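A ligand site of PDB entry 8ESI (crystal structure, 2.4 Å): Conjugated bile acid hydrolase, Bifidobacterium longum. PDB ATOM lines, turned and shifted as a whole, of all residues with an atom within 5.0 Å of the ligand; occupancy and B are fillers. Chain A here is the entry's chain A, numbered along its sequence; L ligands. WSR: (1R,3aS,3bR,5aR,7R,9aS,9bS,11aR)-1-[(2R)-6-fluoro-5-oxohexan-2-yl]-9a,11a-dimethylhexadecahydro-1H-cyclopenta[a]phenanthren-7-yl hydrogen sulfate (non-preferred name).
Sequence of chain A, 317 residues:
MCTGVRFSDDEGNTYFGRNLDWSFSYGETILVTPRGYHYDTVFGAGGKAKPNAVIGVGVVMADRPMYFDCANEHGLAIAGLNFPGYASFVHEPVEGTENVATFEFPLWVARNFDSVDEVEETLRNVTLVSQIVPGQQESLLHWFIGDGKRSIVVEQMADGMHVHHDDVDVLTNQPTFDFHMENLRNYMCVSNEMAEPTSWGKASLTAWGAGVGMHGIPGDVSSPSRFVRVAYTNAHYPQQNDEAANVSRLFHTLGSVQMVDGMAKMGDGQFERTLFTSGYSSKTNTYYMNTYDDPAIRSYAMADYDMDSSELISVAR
The side-chain sulfur (SG) of Cys 2 is bonded to a carbon (C1) of the ligand, 1.8 Å away. An oxygen (O1) of the ligand is in hydrogen-bond range of the backbone NH of Asn 82, at 2.6 Å. ND2 of Asn 173 sits at hydrogen-bond distance from O1 of the ligand, 3.1 Å away.
The backbone NH (N) of Cys 2 sits at hydrogen-bond distance from the side-chain amide oxygen (OD1) of Asn 173 (3.0 Å). The backbone NH (N) of Asp 21 sits at hydrogen-bond distance from the side-chain sulfur (SG) of Cys 2 (3.2 Å). SG of Cys 2 lies within hydrogen-bond range of NH2 of Arg 18, 3.5 Å away. The side-chain amide nitrogen (ND2) of Asn 173 is in hydrogen-bond range of the backbone carbonyl oxygen (O) of Asn 82 (3.1 Å). The side-chain hydroxyl (OH) of Tyr 26 sits at hydrogen-bond distance from the indole nitrogen (NE1) of Trp 22. The backbone carbonyl oxygen (O) of Phe 68 sits at hydrogen-bond distance from the backbone NH (N) of Gly 80 (3.1 Å). O of Phe 68 lies within hydrogen-bond range of NH1 of Arg 18 (3.0 Å). The backbone NH (N) of Met 66 is in hydrogen-bond range of the backbone carbonyl oxygen (O) of Val 59, at 2.8 Å.
O of Gln 131 sits close to O4 of the ligand, at 3.5 Å. O of Asp 21 touches C1 of the ligand (3.2 Å). Trp 22 touches the ligand. Tyr 26 touches the ligand. Val 59 touches the ligand (CG2 to C20, 3.6 Å). CE of Met 66 touches C14 of the ligand, 3.5 Å away. Phe 68 touches the ligand. O of Gly 80 touches C8 of the ligand, 3.9 Å away. C of Leu 81 touches O1 of the ligand, 3.6 Å away. OG1 of Thr 102 touches O4 of the ligand, 3.9 Å away. Phe 103 touches the ligand. O of Gln 137 touches O3 of the ligand (3.6 Å). Ser 139 touches the ligand. Of the 24 residues printed, 16 come within 4 Å of the ligand.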
ATOM      1  N   CYS A   2       5.380   5.480  14.416  1.00  0.00           N
ATOM      2  CA  CYS A   2       4.708   4.252  14.000  1.00  0.00           C
ATOM      3  C   CYS A   2       3.412   4.562  13.281  1.00  0.00           C
ATOM      4  O   CYS A   2       2.909   5.689  13.321  1.00  0.00           O
ATOM      5  CB  CYS A   2       4.437   3.353  15.189  1.00  0.00           C
ATOM      6  SG  CYS A   2       5.892   2.517  15.814  1.00  0.00           S
ATOM      7  N   ARG A  18       1.004  -2.912  11.420  1.00  0.00           N
ATOM      8  CA  ARG A  18       1.634  -1.690  11.907  1.00  0.00           C
ATOM      9  C   ARG A  18       3.114  -1.706  11.550  1.00  0.00           C
ATOM     10  O   ARG A  18       3.723  -2.759  11.393  1.00  0.00           O
ATOM     11  CB  ARG A  18       1.468  -1.524  13.420  1.00  0.00           C
ATOM     12  CG  ARG A  18       1.942  -2.709  14.268  1.00  0.00           C
ATOM     13  CD  ARG A  18       3.399  -2.563  14.720  1.00  0.00           C
ATOM     14  NE  ARG A  18       3.680  -1.299  15.389  1.00  0.00           N
ATOM     15  CZ  ARG A  18       3.429  -1.055  16.664  1.00  0.00           C
ATOM     16  NH1 ARG A  18       2.850  -1.963  17.446  1.00  0.00           N
ATOM     17  NH2 ARG A  18       3.769   0.124  17.179  1.00  0.00           N
ATOM     18  N   ASN A  19       3.668  -0.505  11.405  1.00  0.00           N
ATOM     19  CA  ASN A  19       5.103  -0.306  11.334  1.00  0.00           C
ATOM     20  C   ASN A  19       5.641   0.009  12.723  1.00  0.00           C
ATOM     21  O   ASN A  19       4.965   0.647  13.528  1.00  0.00           O
ATOM     22  CB  ASN A  19       5.452   0.853  10.386  1.00  0.00           C
ATOM     23  CG  ASN A  19       5.262   0.499   8.943  1.00  0.00           C
ATOM     24  OD1 ASN A  19       5.296  -0.675   8.570  1.00  0.00           O
ATOM     25  ND2 ASN A  19       5.066   1.513   8.100  1.00  0.00           N
ATOM     26  N   LEU A  20       6.856  -0.443  12.988  1.00  0.00           N
ATOM     27  CA  LEU A  20       7.557  -0.078  14.219  1.00  0.00           C
ATOM     28  C   LEU A  20       8.726   0.825  13.858  1.00  0.00           C
ATOM     29  O   LEU A  20       9.700   0.385  13.250  1.00  0.00           O
ATOM     30  CB  LEU A  20       8.039  -1.309  14.988  1.00  0.00           C
ATOM     31  CG  LEU A  20       8.407  -0.910  16.417  1.00  0.00           C
ATOM     32  CD1 LEU A  20       7.317  -1.300  17.402  1.00  0.00           C
ATOM     33  CD2 LEU A  20       9.759  -1.472  16.824  1.00  0.00           C
ATOM     34  N   ASP A  21       8.612   2.097  14.237  1.00  0.00           N
ATOM     35  CA  ASP A  21       9.643   3.102  13.980  1.00  0.00           C
ATOM     36  C   ASP A  21      10.327   3.444  15.291  1.00  0.00           C
ATOM     37  O   ASP A  21       9.676   3.917  16.235  1.00  0.00           O
ATOM     38  CB  ASP A  21       9.042   4.354  13.337  1.00  0.00           C
ATOM     39  CG  ASP A  21       8.290   4.052  12.062  1.00  0.00           C
ATOM     40  OD1 ASP A  21       8.625   3.054  11.388  1.00  0.00           O
ATOM     41  OD2 ASP A  21       7.347   4.813  11.731  1.00  0.00           O
ATOM     42  N   TRP A  22      11.623   3.188  15.367  1.00  0.00           N
ATOM     43  CA  TRP A  22      12.398   3.456  16.567  1.00  0.00           C
ATOM     44  C   TRP A  22      13.871   3.506  16.192  1.00  0.00           C
ATOM     45  O   TRP A  22      14.258   3.238  15.052  1.00  0.00           O
ATOM     46  CB  TRP A  22      12.135   2.402  17.654  1.00  0.00           C
ATOM     47  CG  TRP A  22      12.224   2.914  19.060  1.00  0.00           C
ATOM     48  CD1 TRP A  22      13.008   2.417  20.069  1.00  0.00           C
ATOM     49  CD2 TRP A  22      11.512   4.029  19.623  1.00  0.00           C
ATOM     50  NE1 TRP A  22      12.828   3.147  21.213  1.00  0.00           N
ATOM     51  CE2 TRP A  22      11.909   4.143  20.967  1.00  0.00           C
ATOM     52  CE3 TRP A  22      10.577   4.942  19.122  1.00  0.00           C
ATOM     53  CZ2 TRP A  22      11.415   5.126  21.820  1.00  0.00           C
ATOM     54  CZ3 TRP A  22      10.084   5.911  19.966  1.00  0.00           C
ATOM     55  CH2 TRP A  22      10.499   6.007  21.297  1.00  0.00           C
ATOM     56  N   TYR A  26      14.036  -3.874  21.055  1.00  0.00           N
ATOM     57  CA  TYR A  26      13.916  -4.384  22.415  1.00  0.00           C
ATOM     58  C   TYR A  26      14.075  -5.893  22.486  1.00  0.00           C
ATOM     59  O   TYR A  26      13.888  -6.480  23.563  1.00  0.00           O
ATOM     60  CB  TYR A  26      12.573  -3.974  23.024  1.00  0.00           C
ATOM     61  CG  TYR A  26      12.422  -2.486  23.255  1.00  0.00           C
ATOM     62  CD1 TYR A  26      11.993  -1.642  22.237  1.00  0.00           C
ATOM     63  CD2 TYR A  26      12.690  -1.927  24.497  1.00  0.00           C
ATOM     64  CE1 TYR A  26      11.849  -0.285  22.439  1.00  0.00           C
ATOM     65  CE2 TYR A  26      12.551  -0.564  24.711  1.00  0.00           C
ATOM     66  CZ  TYR A  26      12.134   0.250  23.689  1.00  0.00           C
ATOM     67  OH  TYR A  26      11.987   1.608  23.901  1.00  0.00           O
ATOM     68  N   VAL A  59       7.405  -8.808  23.919  1.00  0.00           N
ATOM     69  CA  VAL A  59       8.456  -9.313  24.800  1.00  0.00           C
ATOM     70  C   VAL A  59       7.810  -9.963  26.007  1.00  0.00           C
ATOM     71  O   VAL A  59       6.633  -9.751  26.317  1.00  0.00           O
ATOM     72  CB  VAL A  59       9.427  -8.194  25.247  1.00  0.00           C
ATOM     73  CG1 VAL A  59      10.248  -7.697  24.083  1.00  0.00           C
ATOM     74  CG2 VAL A  59       8.653  -7.045  25.891  1.00  0.00           C
ATOM     75  N   MET A  61       8.157 -10.312  30.052  1.00  0.00           N
ATOM     76  CA  MET A  61       8.724  -9.720  31.259  1.00  0.00           C
ATOM     77  C   MET A  61       7.956 -10.245  32.455  1.00  0.00           C
ATOM     78  O   MET A  61       6.735 -10.090  32.531  1.00  0.00           O
ATOM     79  CB  MET A  61       8.673  -8.190  31.214  1.00  0.00           C
ATOM     80  CG  MET A  61       9.559  -7.564  30.148  1.00  0.00           C
ATOM     81  SD  MET A  61       9.650  -5.773  30.250  1.00  0.00           S
ATOM     82  CE  MET A  61      11.207  -5.455  29.436  1.00  0.00           C
ATOM     83  N   MET A  66       3.958  -9.205  26.985  1.00  0.00           N
ATOM     84  CA  MET A  66       3.750  -7.763  26.817  1.00  0.00           C
ATOM     85  C   MET A  66       3.865  -7.449  25.332  1.00  0.00           C
ATOM     86  O   MET A  66       4.957  -7.211  24.806  1.00  0.00           O
ATOM     87  CB  MET A  66       4.737  -6.993  27.669  1.00  0.00           C
ATOM     88  CG  MET A  66       5.012  -7.677  29.002  1.00  0.00           C
ATOM     89  SD  MET A  66       4.990  -6.569  30.417  1.00  0.00           S
ATOM     90  CE  MET A  66       6.106  -5.284  29.869  1.00  0.00           C
ATOM     91  N   TYR A  67       2.716  -7.439  24.658  1.00  0.00           N
ATOM     92  CA  TYR A  67       2.676  -7.337  23.209  1.00  0.00           C
ATOM     93  C   TYR A  67       2.832  -5.900  22.746  1.00  0.00           C
ATOM     94  O   TYR A  67       2.306  -4.968  23.357  1.00  0.00           O
ATOM     95  CB  TYR A  67       1.341  -7.889  22.685  1.00  0.00           C
ATOM     96  CG  TYR A  67       1.269  -9.395  22.641  1.00  0.00           C
ATOM     97  CD1 TYR A  67       1.861 -10.112  21.621  1.00  0.00           C
ATOM     98  CD2 TYR A  67       0.584 -10.096  23.625  1.00  0.00           C
ATOM     99  CE1 TYR A  67       1.791 -11.490  21.579  1.00  0.00           C
ATOM    100  CE2 TYR A  67       0.503 -11.480  23.590  1.00  0.00           C
ATOM    101  CZ  TYR A  67       1.103 -12.169  22.560  1.00  0.00           C
ATOM    102  OH  TYR A  67       1.027 -13.540  22.516  1.00  0.00           O
ATOM    103  N   PHE A  68       3.578  -5.726  21.645  1.00  0.00           N
ATOM    104  CA  PHE A  68       3.527  -4.480  20.888  1.00  0.00           C
ATOM    105  C   PHE A  68       2.250  -4.406  20.068  1.00  0.00           C
ATOM    106  O   PHE A  68       1.694  -3.327  19.880  1.00  0.00           O
ATOM    107  CB  PHE A  68       4.735  -4.357  19.956  1.00  0.00           C
ATOM    108  CG  PHE A  68       6.073  -4.230  20.643  1.00  0.00           C
ATOM    109  CD1 PHE A  68       6.211  -4.456  22.008  1.00  0.00           C
ATOM    110  CD2 PHE A  68       7.206  -3.903  19.912  1.00  0.00           C
ATOM    111  CE1 PHE A  68       7.445  -4.351  22.619  1.00  0.00           C
ATOM    112  CE2 PHE A  68       8.435  -3.791  20.520  1.00  0.00           C
ATOM    113  CZ  PHE A  68       8.559  -4.015  21.880  1.00  0.00           C
ATOM    114  N   GLY A  80      -0.253  -0.938  19.988  1.00  0.00           N
ATOM    115  CA  GLY A  80       0.072   0.181  20.854  1.00  0.00           C
ATOM    116  C   GLY A  80       1.118   1.066  20.196  1.00  0.00           C
ATOM    117  O   GLY A  80       2.153   0.592  19.739  1.00  0.00           O
ATOM    118  N   LEU A  81       0.817   2.368  20.145  1.00  0.00           N
ATOM    119  CA  LEU A  81       1.659   3.347  19.482  1.00  0.00           C
ATOM    120  C   LEU A  81       1.995   4.461  20.459  1.00  0.00           C
ATOM    121  O   LEU A  81       1.196   4.776  21.352  1.00  0.00           O
ATOM    122  CB  LEU A  81       0.974   3.909  18.225  1.00  0.00           C
ATOM    123  CG  LEU A  81       0.994   3.048  16.950  1.00  0.00           C
ATOM    124  CD1 LEU A  81       0.080   1.829  17.075  1.00  0.00           C
ATOM    125  CD2 LEU A  81       0.601   3.874  15.723  1.00  0.00           C
ATOM    126  N   ASN A  82       3.173   5.053  20.286  1.00  0.00           N
ATOM    127  CA  ASN A  82       3.667   6.022  21.256  1.00  0.00           C
ATOM    128  C   ASN A  82       2.799   7.282  21.284  1.00  0.00           C
ATOM    129  O   ASN A  82       2.331   7.752  20.250  1.00  0.00           O
ATOM    130  CB  ASN A  82       5.115   6.406  20.951  1.00  0.00           C
ATOM    131  CG  ASN A  82       5.927   6.676  22.197  1.00  0.00           C
ATOM    132  OD1 ASN A  82       5.578   6.222  23.290  1.00  0.00           O
ATOM    133  ND2 ASN A  82       7.019   7.418  22.046  1.00  0.00           N
ATOM    134  N   THR A 102      -1.475  -0.790  31.853  1.00  0.00           N
ATOM    135  CA  THR A 102      -1.210  -0.373  30.478  1.00  0.00           C
ATOM    136  C   THR A 102      -0.477  -1.448  29.685  1.00  0.00           C
ATOM    137  O   THR A 102      -0.802  -1.703  28.526  1.00  0.00           O
ATOM    138  CB  THR A 102      -0.422   0.932  30.461  1.00  0.00           C
ATOM    139  OG1 THR A 102       0.797   0.763  31.194  1.00  0.00           O
ATOM    140  CG2 THR A 102      -1.230   2.063  31.084  1.00  0.00           C
ATOM    141  N   PHE A 103       0.501  -2.113  30.309  1.00  0.00           N
ATOM    142  CA  PHE A 103       1.288  -3.116  29.583  1.00  0.00           C
ATOM    143  C   PHE A 103       0.489  -4.378  29.294  1.00  0.00           C
ATOM    144  O   PHE A 103       0.856  -5.130  28.378  1.00  0.00           O
ATOM    145  CB  PHE A 103       2.558  -3.462  30.359  1.00  0.00           C
ATOM    146  CG  PHE A 103       2.326  -3.904  31.780  1.00  0.00           C
ATOM    147  CD1 PHE A 103       1.849  -5.170  32.064  1.00  0.00           C
ATOM    148  CD2 PHE A 103       2.594  -3.043  32.828  1.00  0.00           C
ATOM    149  CE1 PHE A 103       1.634  -5.574  33.371  1.00  0.00           C
ATOM    150  CE2 PHE A 103       2.386  -3.441  34.137  1.00  0.00           C
ATOM    151  CZ  PHE A 103       1.913  -4.707  34.411  1.00  0.00           C
ATOM    152  N   GLN A 131       1.249   1.331  35.841  1.00  0.00           N
ATOM    153  CA  GLN A 131       2.101   0.840  36.917  1.00  0.00           C
ATOM    154  C   GLN A 131       3.555   0.984  36.485  1.00  0.00           C
ATOM    155  O   GLN A 131       4.016   0.275  35.577  1.00  0.00           O
ATOM    156  CB  GLN A 131       1.764  -0.617  37.244  1.00  0.00           C
ATOM    157  CG  GLN A 131       2.441  -1.163  38.486  1.00  0.00           C
ATOM    158  CD  GLN A 131       1.998  -2.583  38.804  1.00  0.00           C
ATOM    159  OE1 GLN A 131       1.140  -2.804  39.656  1.00  0.00           O
ATOM    160  NE2 GLN A 131       2.601  -3.550  38.117  1.00  0.00           N
ATOM    161  N   VAL A 133       7.778   1.147  36.937  1.00  0.00           N
ATOM    162  CA  VAL A 133       8.901   0.511  37.610  1.00  0.00           C
ATOM    163  C   VAL A 133       9.933   1.596  37.900  1.00  0.00           C
ATOM    164  O   VAL A 133       9.919   2.645  37.236  1.00  0.00           O
ATOM    165  CB  VAL A 133       9.490  -0.629  36.772  1.00  0.00           C
ATOM    166  CG1 VAL A 133       8.382  -1.495  36.193  1.00  0.00           C
ATOM    167  CG2 VAL A 133      10.383  -0.077  35.661  1.00  0.00           C
ATOM    168  N   GLN A 137      11.403   4.133  32.249  1.00  0.00           N
ATOM    169  CA  GLN A 137      10.415   5.209  32.205  1.00  0.00           C
ATOM    170  C   GLN A 137       9.037   4.633  31.891  1.00  0.00           C
ATOM    171  O   GLN A 137       8.911   3.569  31.272  1.00  0.00           O
ATOM    172  CB  GLN A 137      10.804   6.252  31.164  1.00  0.00           C
ATOM    173  CG  GLN A 137      12.269   6.657  31.193  1.00  0.00           C
ATOM    174  CD  GLN A 137      12.763   7.140  29.840  1.00  0.00           C
ATOM    175  OE1 GLN A 137      12.008   7.176  28.867  1.00  0.00           O
ATOM    176  NE2 GLN A 137      14.027   7.522  29.768  1.00  0.00           N
ATOM    177  N   GLU A 138       8.007   5.363  32.307  1.00  0.00           N
ATOM    178  CA  GLU A 138       6.642   4.874  32.118  1.00  0.00           C
ATOM    179  C   GLU A 138       6.230   5.017  30.662  1.00  0.00           C
ATOM    180  O   GLU A 138       6.560   6.001  29.987  1.00  0.00           O
ATOM    181  CB  GLU A 138       5.684   5.622  33.048  1.00  0.00           C
ATOM    182  CG  GLU A 138       4.978   6.826  32.446  1.00  0.00           C
ATOM    183  CD  GLU A 138       3.663   7.134  33.147  1.00  0.00           C
ATOM    184  OE1 GLU A 138       2.767   6.273  33.132  1.00  0.00           O
ATOM    185  OE2 GLU A 138       3.539   8.234  33.717  1.00  0.00           O
ATOM    186  N   SER A 139       5.527   4.007  30.164  1.00  0.00           N
ATOM    187  CA  SER A 139       5.109   3.974  28.763  1.00  0.00           C
ATOM    188  C   SER A 139       3.834   4.796  28.596  1.00  0.00           C
ATOM    189  O   SER A 139       2.856   4.604  29.329  1.00  0.00           O
ATOM    190  CB  SER A 139       4.893   2.541  28.290  1.00  0.00           C
ATOM    191  OG  SER A 139       3.528   2.161  28.390  1.00  0.00           O
ATOM    192  N   LEU A 141       1.214   5.524  25.779  1.00  0.00           N
ATOM    193  CA  LEU A 141       0.768   5.061  24.476  1.00  0.00           C
ATOM    194  C   LEU A 141      -0.723   5.357  24.286  1.00  0.00           C
ATOM    195  O   LEU A 141      -1.453   5.684  25.224  1.00  0.00           O
ATOM    196  CB  LEU A 141       1.022   3.559  24.293  1.00  0.00           C
ATOM    197  CG  LEU A 141       2.369   2.963  24.723  1.00  0.00           C
ATOM    198  CD1 LEU A 141       2.362   1.456  24.500  1.00  0.00           C
ATOM    199  CD2 LEU A 141       3.525   3.607  23.985  1.00  0.00           C
ATOM    200  N   ASN A 173       1.032   8.802  15.481  1.00  0.00           N
ATOM    201  CA  ASN A 173       1.393   9.279  16.816  1.00  0.00           C
ATOM    202  C   ASN A 173       0.713  10.598  17.161  1.00  0.00           C
ATOM    203  O   ASN A 173      -0.479  10.789  16.861  1.00  0.00           O
ATOM    204  CB  ASN A 173       2.918   9.412  16.931  1.00  0.00           C
ATOM    205  CG  ASN A 173       3.635   8.116  16.576  1.00  0.00           C
ATOM    206  OD1 ASN A 173       4.193   7.981  15.476  1.00  0.00           O
ATOM    207  ND2 ASN A 173       3.619   7.156  17.499  1.00  0.00           N
HETATM  208  C4  WSR L   1       6.750   3.219  20.542  1.00  0.00           C
HETATM  209  C5  WSR L   1       7.599   2.235  21.358  1.00  0.00           C
HETATM  210  C6  WSR L   1       8.740   2.992  22.032  1.00  0.00           C
HETATM  211  C7  WSR L   1       6.720   1.457  22.364  1.00  0.00           C
HETATM  212  C8  WSR L   1       5.503   0.761  21.690  1.00  0.00           C
HETATM  213  C10 WSR L   1       6.073  -0.369  23.728  1.00  0.00           C
HETATM  214  C13 WSR L   1       5.279  -3.436  25.980  1.00  0.00           C
HETATM  215  C15 WSR L   1       5.296  -2.100  28.124  1.00  0.00           C
HETATM  216  C17 WSR L   1       7.373  -1.007  28.943  1.00  0.00           C
HETATM  217  C20 WSR L   1       8.348  -3.419  26.067  1.00  0.00           C
HETATM  218  C21 WSR L   1       7.172  -1.184  25.833  1.00  0.00           C
HETATM  219  C22 WSR L   1       8.428  -0.402  25.417  1.00  0.00           C
HETATM  220  C24 WSR L   1       7.345   0.336  23.240  1.00  0.00           C
HETATM  221  C1  WSR L   1       6.558   3.770  16.897  1.00  0.00           C
HETATM  222  C11 WSR L   1       6.316  -1.590  24.615  1.00  0.00           C
HETATM  223  C12 WSR L   1       5.022  -2.250  25.060  1.00  0.00           C
HETATM  224  C14 WSR L   1       6.108  -3.012  27.198  1.00  0.00           C
HETATM  225  C16 WSR L   1       6.078  -1.668  29.346  1.00  0.00           C
HETATM  226  C18 WSR L   1       8.199  -1.934  28.055  1.00  0.00           C
HETATM  227  C19 WSR L   1       7.459  -2.381  26.775  1.00  0.00           C
HETATM  228  C2  WSR L   1       5.904   3.767  18.208  1.00  0.00           C
HETATM  229  C23 WSR L   1       8.112   0.778  24.487  1.00  0.00           C
HETATM  230  C25 WSR L   1       8.218  -0.590  22.368  1.00  0.00           C
HETATM  231  C3  WSR L   1       6.349   2.712  19.163  1.00  0.00           C
HETATM  232  C9  WSR L   1       5.245  -0.545  22.459  1.00  0.00           C
HETATM  233  O1  WSR L   1       5.042   4.562  18.498  1.00  0.00           O
HETATM  234  O2  WSR L   1       5.263  -0.696  30.117  1.00  0.00           O
HETATM  235  O3  WSR L   1       6.863   0.660  31.406  1.00  0.00           O
HETATM  236  O4  WSR L   1       4.589   0.411  32.152  1.00  0.00           O
HETATM  237  O5  WSR L   1       6.101  -1.471  32.243  1.00  0.00           O
HETATM  238  S1  WSR L   1       5.737  -0.241  31.568  1.00  0.00           S
